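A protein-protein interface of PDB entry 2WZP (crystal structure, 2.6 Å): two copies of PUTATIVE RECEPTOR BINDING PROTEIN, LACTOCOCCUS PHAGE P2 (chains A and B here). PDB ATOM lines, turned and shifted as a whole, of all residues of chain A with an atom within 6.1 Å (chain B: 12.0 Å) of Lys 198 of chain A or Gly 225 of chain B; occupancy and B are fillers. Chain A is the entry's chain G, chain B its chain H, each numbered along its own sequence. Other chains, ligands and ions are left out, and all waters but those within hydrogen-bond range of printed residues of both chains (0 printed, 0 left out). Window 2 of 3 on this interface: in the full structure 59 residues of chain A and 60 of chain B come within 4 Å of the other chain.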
ATOM      1  N   ILE A 196     -14.076   8.945  31.530  1.00  0.00           N
ATOM      2  CA  ILE A 196     -12.788   9.283  30.928  1.00  0.00           C
ATOM      3  C   ILE A 196     -12.965   9.745  29.483  1.00  0.00           C
ATOM      4  O   ILE A 196     -13.879   9.280  28.801  1.00  0.00           O
ATOM      5  CB  ILE A 196     -11.768   8.103  31.065  1.00  0.00           C
ATOM      6  CG1 ILE A 196     -10.320   8.528  30.699  1.00  0.00           C
ATOM      7  CG2 ILE A 196     -12.209   6.867  30.258  1.00  0.00           C
ATOM      8  CD1 ILE A 196      -9.529   9.280  31.745  1.00  0.00           C
ATOM      9  N   GLN A 197     -12.084  10.645  29.019  1.00  0.00           N
ATOM     10  CA  GLN A 197     -12.107  11.131  27.648  1.00  0.00           C
ATOM     11  C   GLN A 197     -10.813  10.781  26.952  1.00  0.00           C
ATOM     12  O   GLN A 197      -9.775  10.679  27.607  1.00  0.00           O
ATOM     13  CB  GLN A 197     -12.313  12.647  27.612  1.00  0.00           C
ATOM     14  CG  GLN A 197     -13.681  13.111  28.098  1.00  0.00           C
ATOM     15  CD  GLN A 197     -13.695  14.599  28.342  1.00  0.00           C
ATOM     16  OE1 GLN A 197     -13.470  15.404  27.432  1.00  0.00           O
ATOM     17  NE2 GLN A 197     -13.954  14.999  29.584  1.00  0.00           N
ATOM     18  N   LYS A 198     -10.868  10.619  25.618  1.00  0.00           N
ATOM     19  CA  LYS A 198      -9.696  10.338  24.789  1.00  0.00           C
ATOM     20  C   LYS A 198      -8.651  11.441  24.951  1.00  0.00           C
ATOM     21  O   LYS A 198      -9.010  12.627  24.961  1.00  0.00           O
ATOM     22  CB  LYS A 198     -10.094  10.199  23.310  1.00  0.00           C
ATOM     23  CG  LYS A 198     -10.820  11.392  22.680  1.00  0.00           C
ATOM     24  CD  LYS A 198     -12.075  10.889  21.973  1.00  0.00           C
ATOM     25  CE  LYS A 198     -12.553  11.744  20.843  1.00  0.00           C
ATOM     26  NZ  LYS A 198     -12.820  10.910  19.638  1.00  0.00           N
ATOM     27  N   GLY A 199      -7.395  11.035  25.126  1.00  0.00           N
ATOM     28  CA  GLY A 199      -6.271  11.950  25.303  1.00  0.00           C
ATOM     29  C   GLY A 199      -6.042  12.409  26.723  1.00  0.00           C
ATOM     30  O   GLY A 199      -5.043  13.077  26.999  1.00  0.00           O
ATOM     31  N   TRP A 200      -6.968  12.060  27.627  1.00  0.00           N
ATOM     32  CA  TRP A 200      -6.867  12.447  29.022  1.00  0.00           C
ATOM     33  C   TRP A 200      -6.037  11.485  29.826  1.00  0.00           C
ATOM     34  O   TRP A 200      -6.067  10.276  29.593  1.00  0.00           O
ATOM     35  CB  TRP A 200      -8.247  12.688  29.660  1.00  0.00           C
ATOM     36  CG  TRP A 200      -8.902  13.949  29.160  1.00  0.00           C
ATOM     37  CD1 TRP A 200      -9.313  14.201  27.884  1.00  0.00           C
ATOM     38  CD2 TRP A 200      -9.114  15.164  29.895  1.00  0.00           C
ATOM     39  NE1 TRP A 200      -9.815  15.475  27.788  1.00  0.00           N
ATOM     40  CE2 TRP A 200      -9.688  16.097  29.002  1.00  0.00           C
ATOM     41  CE3 TRP A 200      -8.857  15.564  31.219  1.00  0.00           C
ATOM     42  CZ2 TRP A 200     -10.041  17.396  29.397  1.00  0.00           C
ATOM     43  CZ3 TRP A 200      -9.210  16.851  31.611  1.00  0.00           C
ATOM     44  CH2 TRP A 200      -9.792  17.751  30.706  1.00  0.00           C
ATOM     45  N   HIS A 231      -7.031   1.499  23.995  1.00  0.00           N
ATOM     46  CA  HIS A 231      -5.606   1.450  24.242  1.00  0.00           C
ATOM     47  C   HIS A 231      -5.219   2.522  25.223  1.00  0.00           C
ATOM     48  O   HIS A 231      -5.912   3.518  25.348  1.00  0.00           O
ATOM     49  CB  HIS A 231      -4.717   1.380  22.980  1.00  0.00           C
ATOM     50  CG  HIS A 231      -4.199   2.688  22.462  1.00  0.00           C
ATOM     51  ND1 HIS A 231      -4.872   3.379  21.482  1.00  0.00           N
ATOM     52  CD2 HIS A 231      -3.042   3.337  22.736  1.00  0.00           C
ATOM     53  CE1 HIS A 231      -4.121   4.428  21.193  1.00  0.00           C
ATOM     54  NE2 HIS A 231      -3.020   4.456  21.938  1.00  0.00           N
ATOM     55  N   THR A 241      -2.095   7.620  29.703  1.00  0.00           N
ATOM     56  CA  THR A 241      -3.033   8.371  28.874  1.00  0.00           C
ATOM     57  C   THR A 241      -4.078   7.428  28.267  1.00  0.00           C
ATOM     58  O   THR A 241      -3.720   6.416  27.670  1.00  0.00           O
ATOM     59  CB  THR A 241      -2.284   9.164  27.787  1.00  0.00           C
ATOM     60  OG1 THR A 241      -1.202   9.877  28.382  1.00  0.00           O
ATOM     61  CG2 THR A 241      -3.195  10.126  27.033  1.00  0.00           C
ATOM     62  N   TRP A 242      -5.367   7.787  28.398  1.00  0.00           N
ATOM     63  CA  TRP A 242      -6.471   7.014  27.833  1.00  0.00           C
ATOM     64  C   TRP A 242      -6.599   7.293  26.349  1.00  0.00           C
ATOM     65  O   TRP A 242      -6.700   8.450  25.933  1.00  0.00           O
ATOM     66  CB  TRP A 242      -7.790   7.340  28.536  1.00  0.00           C
ATOM     67  CG  TRP A 242      -8.971   6.573  27.994  1.00  0.00           C
ATOM     68  CD1 TRP A 242      -9.943   7.044  27.158  1.00  0.00           C
ATOM     69  CD2 TRP A 242      -9.285   5.188  28.235  1.00  0.00           C
ATOM     70  NE1 TRP A 242     -10.860   6.051  26.887  1.00  0.00           N
ATOM     71  CE2 TRP A 242     -10.472   4.897  27.523  1.00  0.00           C
ATOM     72  CE3 TRP A 242      -8.688   4.167  28.995  1.00  0.00           C
ATOM     73  CZ2 TRP A 242     -11.067   3.622  27.542  1.00  0.00           C
ATOM     74  CZ3 TRP A 242      -9.284   2.910  29.023  1.00  0.00           C
ATOM     75  CH2 TRP A 242     -10.460   2.649  28.309  1.00  0.00           C
ATOM     76  N   TRP A 243      -6.628   6.234  25.553  1.00  0.00           N
ATOM     77  CA  TRP A 243      -6.790   6.384  24.120  1.00  0.00           C
ATOM     78  C   TRP A 243      -7.917   5.574  23.501  1.00  0.00           C
ATOM     79  O   TRP A 243      -7.932   5.345  22.291  1.00  0.00           O
ATOM     80  CB  TRP A 243      -5.467   6.264  23.376  1.00  0.00           C
ATOM     81  CG  TRP A 243      -4.613   7.486  23.460  1.00  0.00           C
ATOM     82  CD1 TRP A 243      -3.396   7.595  24.067  1.00  0.00           C
ATOM     83  CD2 TRP A 243      -4.906   8.776  22.909  1.00  0.00           C
ATOM     84  NE1 TRP A 243      -2.906   8.869  23.917  1.00  0.00           N
ATOM     85  CE2 TRP A 243      -3.817   9.619  23.217  1.00  0.00           C
ATOM     86  CE3 TRP A 243      -5.990   9.305  22.177  1.00  0.00           C
ATOM     87  CZ2 TRP A 243      -3.783  10.967  22.833  1.00  0.00           C
ATOM     88  CZ3 TRP A 243      -5.954  10.638  21.792  1.00  0.00           C
ATOM     89  CH2 TRP A 243      -4.854  11.450  22.104  1.00  0.00           C
ATOM     90  N   GLY A 244      -8.878   5.196  24.329  1.00  0.00           N
ATOM     91  CA  GLY A 244     -10.105   4.583  23.854  1.00  0.00           C
ATOM     92  C   GLY A 244     -11.076   5.721  23.575  1.00  0.00           C
ATOM     93  O   GLY A 244     -10.705   6.899  23.682  1.00  0.00           O
ATOM     94  N   ALA A 245     -12.333   5.395  23.254  1.00  0.00           N
ATOM     95  CA  ALA A 245     -13.365   6.412  23.048  1.00  0.00           C
ATOM     96  C   ALA A 245     -13.761   7.000  24.410  1.00  0.00           C
ATOM     97  O   ALA A 245     -13.354   6.464  25.447  1.00  0.00           O
ATOM     98  CB  ALA A 245     -14.577   5.775  22.382  1.00  0.00           C
ATOM     99  N   ASN A 246     -14.541   8.093  24.417  1.00  0.00           N
ATOM    100  CA  ASN A 246     -15.009   8.685  25.666  1.00  0.00           C
ATOM    101  C   ASN A 246     -15.940   7.702  26.359  1.00  0.00           C
ATOM    102  O   ASN A 246     -16.816   7.126  25.705  1.00  0.00           O
ATOM    103  CB  ASN A 246     -15.722  10.012  25.417  1.00  0.00           C
ATOM    104  CG  ASN A 246     -14.842  11.112  24.884  1.00  0.00           C
ATOM    105  OD1 ASN A 246     -13.625  10.971  24.754  1.00  0.00           O
ATOM    106  ND2 ASN A 246     -15.442  12.238  24.551  1.00  0.00           N
ATOM    107  N   PHE B 189       3.112   0.575  16.859  1.00  0.00           N
ATOM    108  CA  PHE B 189       2.478   1.265  15.738  1.00  0.00           C
ATOM    109  C   PHE B 189       2.450   2.752  15.960  1.00  0.00           C
ATOM    110  O   PHE B 189       2.180   3.216  17.076  1.00  0.00           O
ATOM    111  CB  PHE B 189       1.042   0.782  15.511  1.00  0.00           C
ATOM    112  CG  PHE B 189       0.901  -0.648  15.076  1.00  0.00           C
ATOM    113  CD1 PHE B 189       1.400  -1.070  13.854  1.00  0.00           C
ATOM    114  CD2 PHE B 189       0.227  -1.568  15.869  1.00  0.00           C
ATOM    115  CE1 PHE B 189       1.256  -2.394  13.446  1.00  0.00           C
ATOM    116  CE2 PHE B 189       0.081  -2.894  15.461  1.00  0.00           C
ATOM    117  CZ  PHE B 189       0.592  -3.296  14.248  1.00  0.00           C
ATOM    118  N   GLY B 191       1.919   6.730  13.381  1.00  0.00           N
ATOM    119  CA  GLY B 191       1.348   7.337  12.186  1.00  0.00           C
ATOM    120  C   GLY B 191      -0.166   7.323  12.182  1.00  0.00           C
ATOM    121  O   GLY B 191      -0.806   7.180  13.231  1.00  0.00           O
ATOM    122  N   SER B 192      -0.741   7.504  10.989  1.00  0.00           N
ATOM    123  CA  SER B 192      -2.183   7.551  10.766  1.00  0.00           C
ATOM    124  C   SER B 192      -2.469   6.961   9.404  1.00  0.00           C
ATOM    125  O   SER B 192      -1.871   7.383   8.417  1.00  0.00           O
ATOM    126  CB  SER B 192      -2.692   8.988  10.844  1.00  0.00           C
ATOM    127  OG  SER B 192      -2.427   9.579  12.105  1.00  0.00           O
ATOM    128  N   GLY B 221      -3.755  -3.803  16.327  1.00  0.00           N
ATOM    129  CA  GLY B 221      -3.559  -2.393  16.626  1.00  0.00           C
ATOM    130  C   GLY B 221      -4.870  -1.726  16.995  1.00  0.00           C
ATOM    131  O   GLY B 221      -5.949  -2.305  16.822  1.00  0.00           O
ATOM    132  N   HIS B 222      -4.788  -0.500  17.476  1.00  0.00           N
ATOM    133  CA  HIS B 222      -5.970   0.237  17.878  1.00  0.00           C
ATOM    134  C   HIS B 222      -6.013   1.635  17.230  1.00  0.00           C
ATOM    135  O   HIS B 222      -4.969   2.183  16.855  1.00  0.00           O
ATOM    136  CB  HIS B 222      -6.008   0.294  19.418  1.00  0.00           C
ATOM    137  CG  HIS B 222      -7.225   0.951  19.967  1.00  0.00           C
ATOM    138  ND1 HIS B 222      -7.157   2.181  20.573  1.00  0.00           N
ATOM    139  CD2 HIS B 222      -8.514   0.548  19.931  1.00  0.00           C
ATOM    140  CE1 HIS B 222      -8.396   2.481  20.913  1.00  0.00           C
ATOM    141  NE2 HIS B 222      -9.250   1.535  20.529  1.00  0.00           N
ATOM    142  N   PHE B 223      -7.219   2.182  17.055  1.00  0.00           N
ATOM    143  CA  PHE B 223      -7.401   3.531  16.529  1.00  0.00           C
ATOM    144  C   PHE B 223      -7.589   4.476  17.690  1.00  0.00           C
ATOM    145  O   PHE B 223      -8.564   4.347  18.431  1.00  0.00           O
ATOM    146  CB  PHE B 223      -8.589   3.601  15.585  1.00  0.00           C
ATOM    147  CG  PHE B 223      -8.364   2.864  14.295  1.00  0.00           C
ATOM    148  CD1 PHE B 223      -7.394   3.292  13.388  1.00  0.00           C
ATOM    149  CD2 PHE B 223      -9.144   1.759  13.966  1.00  0.00           C
ATOM    150  CE1 PHE B 223      -7.198   2.614  12.182  1.00  0.00           C
ATOM    151  CE2 PHE B 223      -8.946   1.079  12.761  1.00  0.00           C
ATOM    152  CZ  PHE B 223      -7.973   1.510  11.878  1.00  0.00           C
ATOM    153  N   ALA B 224      -6.628   5.395  17.878  1.00  0.00           N
ATOM    154  CA  ALA B 224      -6.623   6.352  18.983  1.00  0.00           C
ATOM    155  C   ALA B 224      -7.917   7.156  19.121  1.00  0.00           C
ATOM    156  O   ALA B 224      -8.419   7.720  18.140  1.00  0.00           O
ATOM    157  CB  ALA B 224      -5.439   7.280  18.855  1.00  0.00           C
ATOM    158  N   GLY B 225      -8.457   7.146  20.337  1.00  0.00           N
ATOM    159  CA  GLY B 225      -9.688   7.841  20.691  1.00  0.00           C
ATOM    160  C   GLY B 225     -10.969   7.185  20.214  1.00  0.00           C
ATOM    161  O   GLY B 225     -12.042   7.792  20.300  1.00  0.00           O
ATOM    162  N   ARG B 226     -10.870   5.946  19.702  1.00  0.00           N
ATOM    163  CA  ARG B 226     -12.007   5.189  19.181  1.00  0.00           C
ATOM    164  C   ARG B 226     -12.153   3.837  19.884  1.00  0.00           C
ATOM    165  O   ARG B 226     -11.284   3.441  20.662  1.00  0.00           O
ATOM    166  CB  ARG B 226     -11.843   4.977  17.672  1.00  0.00           C
ATOM    167  CG  ARG B 226     -11.655   6.272  16.890  1.00  0.00           C
ATOM    168  CD  ARG B 226     -11.876   6.078  15.412  1.00  0.00           C
ATOM    169  NE  ARG B 226     -11.809   7.345  14.692  1.00  0.00           N
ATOM    170  CZ  ARG B 226     -12.311   7.540  13.478  1.00  0.00           C
ATOM    171  NH1 ARG B 226     -12.199   8.723  12.889  1.00  0.00           N
ATOM    172  NH2 ARG B 226     -12.940   6.556  12.846  1.00  0.00           N
ATOM    173  N   ASP B 227     -13.259   3.134  19.634  1.00  0.00           N
ATOM    174  CA  ASP B 227     -13.436   1.793  20.193  1.00  0.00           C
ATOM    175  C   ASP B 227     -13.196   0.732  19.103  1.00  0.00           C
ATOM    176  O   ASP B 227     -13.494  -0.455  19.277  1.00  0.00           O
ATOM    177  CB  ASP B 227     -14.765   1.626  20.954  1.00  0.00           C
ATOM    178  CG  ASP B 227     -16.023   2.052  20.238  1.00  0.00           C
ATOM    179  OD1 ASP B 227     -15.982   2.198  18.982  1.00  0.00           O
ATOM    180  OD2 ASP B 227     -17.062   2.237  20.926  1.00  0.00           O
ATOM    181  N   THR B 228     -12.592   1.181  17.993  1.00  0.00           N
ATOM    182  CA  THR B 228     -12.279   0.372  16.821  1.00  0.00           C
ATOM    183  C   THR B 228     -10.821  -0.083  16.766  1.00  0.00           C
ATOM    184  O   THR B 228      -9.923   0.597  17.273  1.00  0.00           O
ATOM    185  CB  THR B 228     -12.720   1.092  15.549  1.00  0.00           C
ATOM    186  OG1 THR B 228     -12.075   2.362  15.486  1.00  0.00           O
ATOM    187  CG2 THR B 228     -14.234   1.267  15.481  1.00  0.00           C
ATOM    188  N   SER B 229     -10.592  -1.229  16.120  1.00  0.00           N
ATOM    189  CA  SER B 229      -9.267  -1.821  16.008  1.00  0.00           C
ATOM    190  C   SER B 229      -8.982  -2.296  14.589  1.00  0.00           C
ATOM    191  O   SER B 229      -9.865  -2.278  13.732  1.00  0.00           O
ATOM    192  CB  SER B 229      -9.154  -2.988  16.983  1.00  0.00           C
ATOM    193  OG  SER B 229     -10.184  -3.941  16.773  1.00  0.00           O
ATOM    194  N   PHE B 230      -7.744  -2.714  14.348  1.00  0.00           N
ATOM    195  CA  PHE B 230      -7.288  -3.255  13.077  1.00  0.00           C
ATOM    196  C   PHE B 230      -6.233  -4.313  13.371  1.00  0.00           C
ATOM    197  O   PHE B 230      -5.799  -4.467  14.515  1.00  0.00           O
ATOM    198  CB  PHE B 230      -6.669  -2.141  12.201  1.00  0.00           C
ATOM    199  CG  PHE B 230      -5.374  -1.563  12.728  1.00  0.00           C
ATOM    200  CD1 PHE B 230      -4.145  -2.081  12.327  1.00  0.00           C
ATOM    201  CD2 PHE B 230      -5.381  -0.501  13.624  1.00  0.00           C
ATOM    202  CE1 PHE B 230      -2.950  -1.557  12.826  1.00  0.00           C
ATOM    203  CE2 PHE B 230      -4.186   0.030  14.113  1.00  0.00           C
ATOM    204  CZ  PHE B 230      -2.978  -0.499  13.705  1.00  0.00           C
ATOM    205  N   THR B 250      -9.591  10.374   5.054  1.00  0.00           N
ATOM    206  CA  THR B 250      -9.277  10.920   6.377  1.00  0.00           C
ATOM    207  C   THR B 250      -8.412   9.948   7.197  1.00  0.00           C
ATOM    208  O   THR B 250      -8.890   8.867   7.557  1.00  0.00           O
ATOM    209  CB  THR B 250     -10.548  11.356   7.124  1.00  0.00           C
ATOM    210  OG1 THR B 250     -11.367  12.155   6.267  1.00  0.00           O
ATOM    211  CG2 THR B 250     -10.231  12.122   8.407  1.00  0.00           C
ATOM    212  N   PRO B 251      -7.151  10.306   7.533  1.00  0.00           N
ATOM    213  CA  PRO B 251      -6.328   9.384   8.317  1.00  0.00           C
ATOM    214  C   PRO B 251      -6.726   9.314   9.789  1.00  0.00           C
ATOM    215  O   PRO B 251      -7.071  10.336  10.396  1.00  0.00           O
ATOM    216  CB  PRO B 251      -4.898   9.914   8.113  1.00  0.00           C
ATOM    217  CG  PRO B 251      -5.000  10.987   7.066  1.00  0.00           C
ATOM    218  CD  PRO B 251      -6.387  11.518   7.195  1.00  0.00           C
ATOM    219  N   ILE B 252      -6.721   8.081  10.339  1.00  0.00           N
ATOM    220  CA  ILE B 252      -7.003   7.783  11.748  1.00  0.00           C
ATOM    221  C   ILE B 252      -5.718   7.258  12.375  1.00  0.00           C
ATOM    222  O   ILE B 252      -5.115   6.296  11.876  1.00  0.00           O
ATOM    223  CB  ILE B 252      -8.176   6.798  12.016  1.00  0.00           C
ATOM    224  CG1 ILE B 252      -9.314   6.900  10.975  1.00  0.00           C
ATOM    225  CG2 ILE B 252      -8.683   6.950  13.463  1.00  0.00           C
ATOM    226  CD1 ILE B 252      -9.956   5.538  10.609  1.00  0.00           C
ATOM    227  N   ALA B 253      -5.328   7.887  13.489  1.00  0.00           N
ATOM    228  CA  ALA B 253      -4.126   7.552  14.245  1.00  0.00           C
ATOM    229  C   ALA B 253      -4.124   6.083  14.690  1.00  0.00           C
ATOM    230  O   ALA B 253      -5.100   5.590  15.273  1.00  0.00           O
ATOM    231  CB  ALA B 253      -3.970   8.484  15.436  1.00  0.00           C
ATOM    232  N   THR B 254      -3.023   5.390  14.361  1.00  0.00           N
ATOM    233  CA  THR B 254      -2.820   3.970  14.626  1.00  0.00           C
ATOM    234  C   THR B 254      -1.762   3.774  15.696  1.00  0.00           C
ATOM    235  O   THR B 254      -0.643   4.286  15.573  1.00  0.00           O
ATOM    236  CB  THR B 254      -2.449   3.248  13.325  1.00  0.00           C
ATOM    237  OG1 THR B 254      -1.399   3.970  12.671  1.00  0.00           O
ATOM    238  CG2 THR B 254      -3.634   3.097  12.394  1.00  0.00           C
ATOM    239  N   ARG B 255      -2.114   3.042  16.757  1.00  0.00           N
ATOM    240  CA  ARG B 255      -1.185   2.790  17.860  1.00  0.00           C
ATOM    241  C   ARG B 255      -1.279   1.339  18.338  1.00  0.00           C
ATOM    242  O   ARG B 255      -2.182   0.602  17.926  1.00  0.00           O
ATOM    243  CB  ARG B 255      -1.481   3.750  19.033  1.00  0.00           C
ATOM    244  CG  ARG B 255      -1.376   5.242  18.731  1.00  0.00           C
ATOM    245  CD  ARG B 255       0.060   5.732  18.553  1.00  0.00           C
ATOM    246  NE  ARG B 255       0.135   7.175  18.304  1.00  0.00           N
ATOM    247  CZ  ARG B 255      -0.004   7.749  17.109  1.00  0.00           C
ATOM    248  NH1 ARG B 255      -0.233   7.006  16.031  1.00  0.00           N
ATOM    249  NH2 ARG B 255       0.084   9.064  16.983  1.00  0.00           N
ATOM    250  N   GLY B 256      -0.361   0.949  19.217  1.00  0.00           N
ATOM    251  CA  GLY B 256      -0.395  -0.375  19.826  1.00  0.00           C
ATOM    252  C   GLY B 256       0.879  -1.174  19.732  1.00  0.00           C
ATOM    253  O   GLY B 256       1.678  -0.983  18.811  1.00  0.00           O
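The side-chain amino group (NZ) of Lys 198 of chain A is in hydrogen-bond range of the backbone carbonyl oxygen (O) of Gly 225 of chain B (3.3 Å).
ND1 of His 231 of chain A lies within hydrogen-bond range of ND1 of His 222 of chain B, at 2.7 Å.
O of Trp 243 of chain A is in hydrogen-bond range of N of Gly 225 of chain B (2.7 Å).
N of Ala 245 of chain A is in hydrogen-bond range of O of Arg 226 of chain B, at 3.4 Å.
O of His 231 of chain A sits at hydrogen-bond distance from N of Trp 243 of chain A, 2.8 Å away.
The backbone carbonyl oxygen (O) of Gly 244 of chain A sits at hydrogen-bond distance from the indole nitrogen (NE1) of Trp 242 of chain A (3.3 Å).
NE1 of Trp 242 of chain A sits at hydrogen-bond distance from O of Ala 245 of chain A (2.9 Å).
O of Arg 226 of chain B lies within hydrogen-bond range of NE2 of His 222 of chain B (2.8 Å).
A ring nitrogen (NE2) of His 222 of chain B lies close to the backbone carbonyl oxygen (O) of Thr 228 of chain B, at 3.5 Å.
The backbone carbonyl oxygen (O) of Ala 253 of chain B lies within hydrogen-bond range of the backbone NH (N) of Ala 224 of chain B (3.0 Å).
CA of Ala 224 of chain B touches CE1 of His 231 of chain A (3.9 Å).
His 231 of chain A touches Arg 255 of chain B.
Trp 243 of chain A touches His 222 of chain B (O to CE1, 3.2 Å).
O of Trp 243 of chain A touches C of Ala 224 of chain B, 3.7 Å away.
Trp 243 of chain A touches Arg 226 of chain B.
Gly 244 of chain A touches His 222 of chain B.
O of Gly 244 of chain A touches CA of Gly 225 of chain B, 3.3 Å away.
O of Arg 226 of chain B touches CA of Gly 244 of chain A (3.6 Å).
CA of Ala 245 of chain A touches O of Gly 225 of chain B (3.3 Å).
No residue of chain B comes within 4 Å of Ile 196 of chain A.
No residue of chain B comes within 4 Å of Gln 197 of chain A.
Lys 198 of chain A touches just one residue of chain B: Gly 225.
No residue of chain B comes within 4 Å of Trp 200 of chain A.
Of chain B, only His 222 (2.7 Å), Ala 224 (3.9 Å) and Arg 255 (3.4 Å) come within 4 Å of His 231 of chain A.
Trp 243 of chain A touches just these residues of chain B: His 222 (3.2 Å), Ala 224 (3.7 Å), Gly 225 (2.7 Å) and Arg 226 (3.96 Å).
Ala 245 of chain A touches just these residues of chain B: Gly 225 (3.3 Å) and Arg 226 (3.4 Å).
Of the printed residues of chain A, His 222 of chain B touches His 231, Trp 243 and Gly 244.
Of the printed residues of chain A, Ala 224 of chain B touches His 231 and Trp 243.
Of the printed residues of chain A, Arg 226 of chain B touches Trp 243 (3.96 Å), Gly 244 (3.6 Å) and Ala 245 (3.4 Å).
Of the printed residues of chain A, Arg 255 of chain B touches His 231 (3.4 Å).
The nearest residue of chain B that does not touch Lys 198 of chain A is Arg 226 of chain B (5.3 Å).
The nearest printed residue of chain A that does not touch His 222 of chain B is Ala 245 of chain A (5.4 Å).
Hydrophobic or aromatic side chains of chain B within 4 Å of the printed part of chain A: His 222 and Ala 224.
Of the 12 printed residues of chain A, 5 touch a printed residue of chain B.
Printed residues of chain A that touch a printed residue of chain B: Lys 198, His 231, Trp 243, Gly 244 and Ala 245.
Hydrophobic or aromatic side chains of chain A within 4 Å of the printed part of chain B: His 231, Trp 243 and Ala 245.
Along chain A the printed residues that touch a printed residue of chain B span positions 198 to 245.
Among the printed residues, 13 pairs touch across the chains.
No position is printed for both chains.
Of the 13 pairs that touch across the chains among the printed residues, none has its exchanged pair printed and touching as well.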
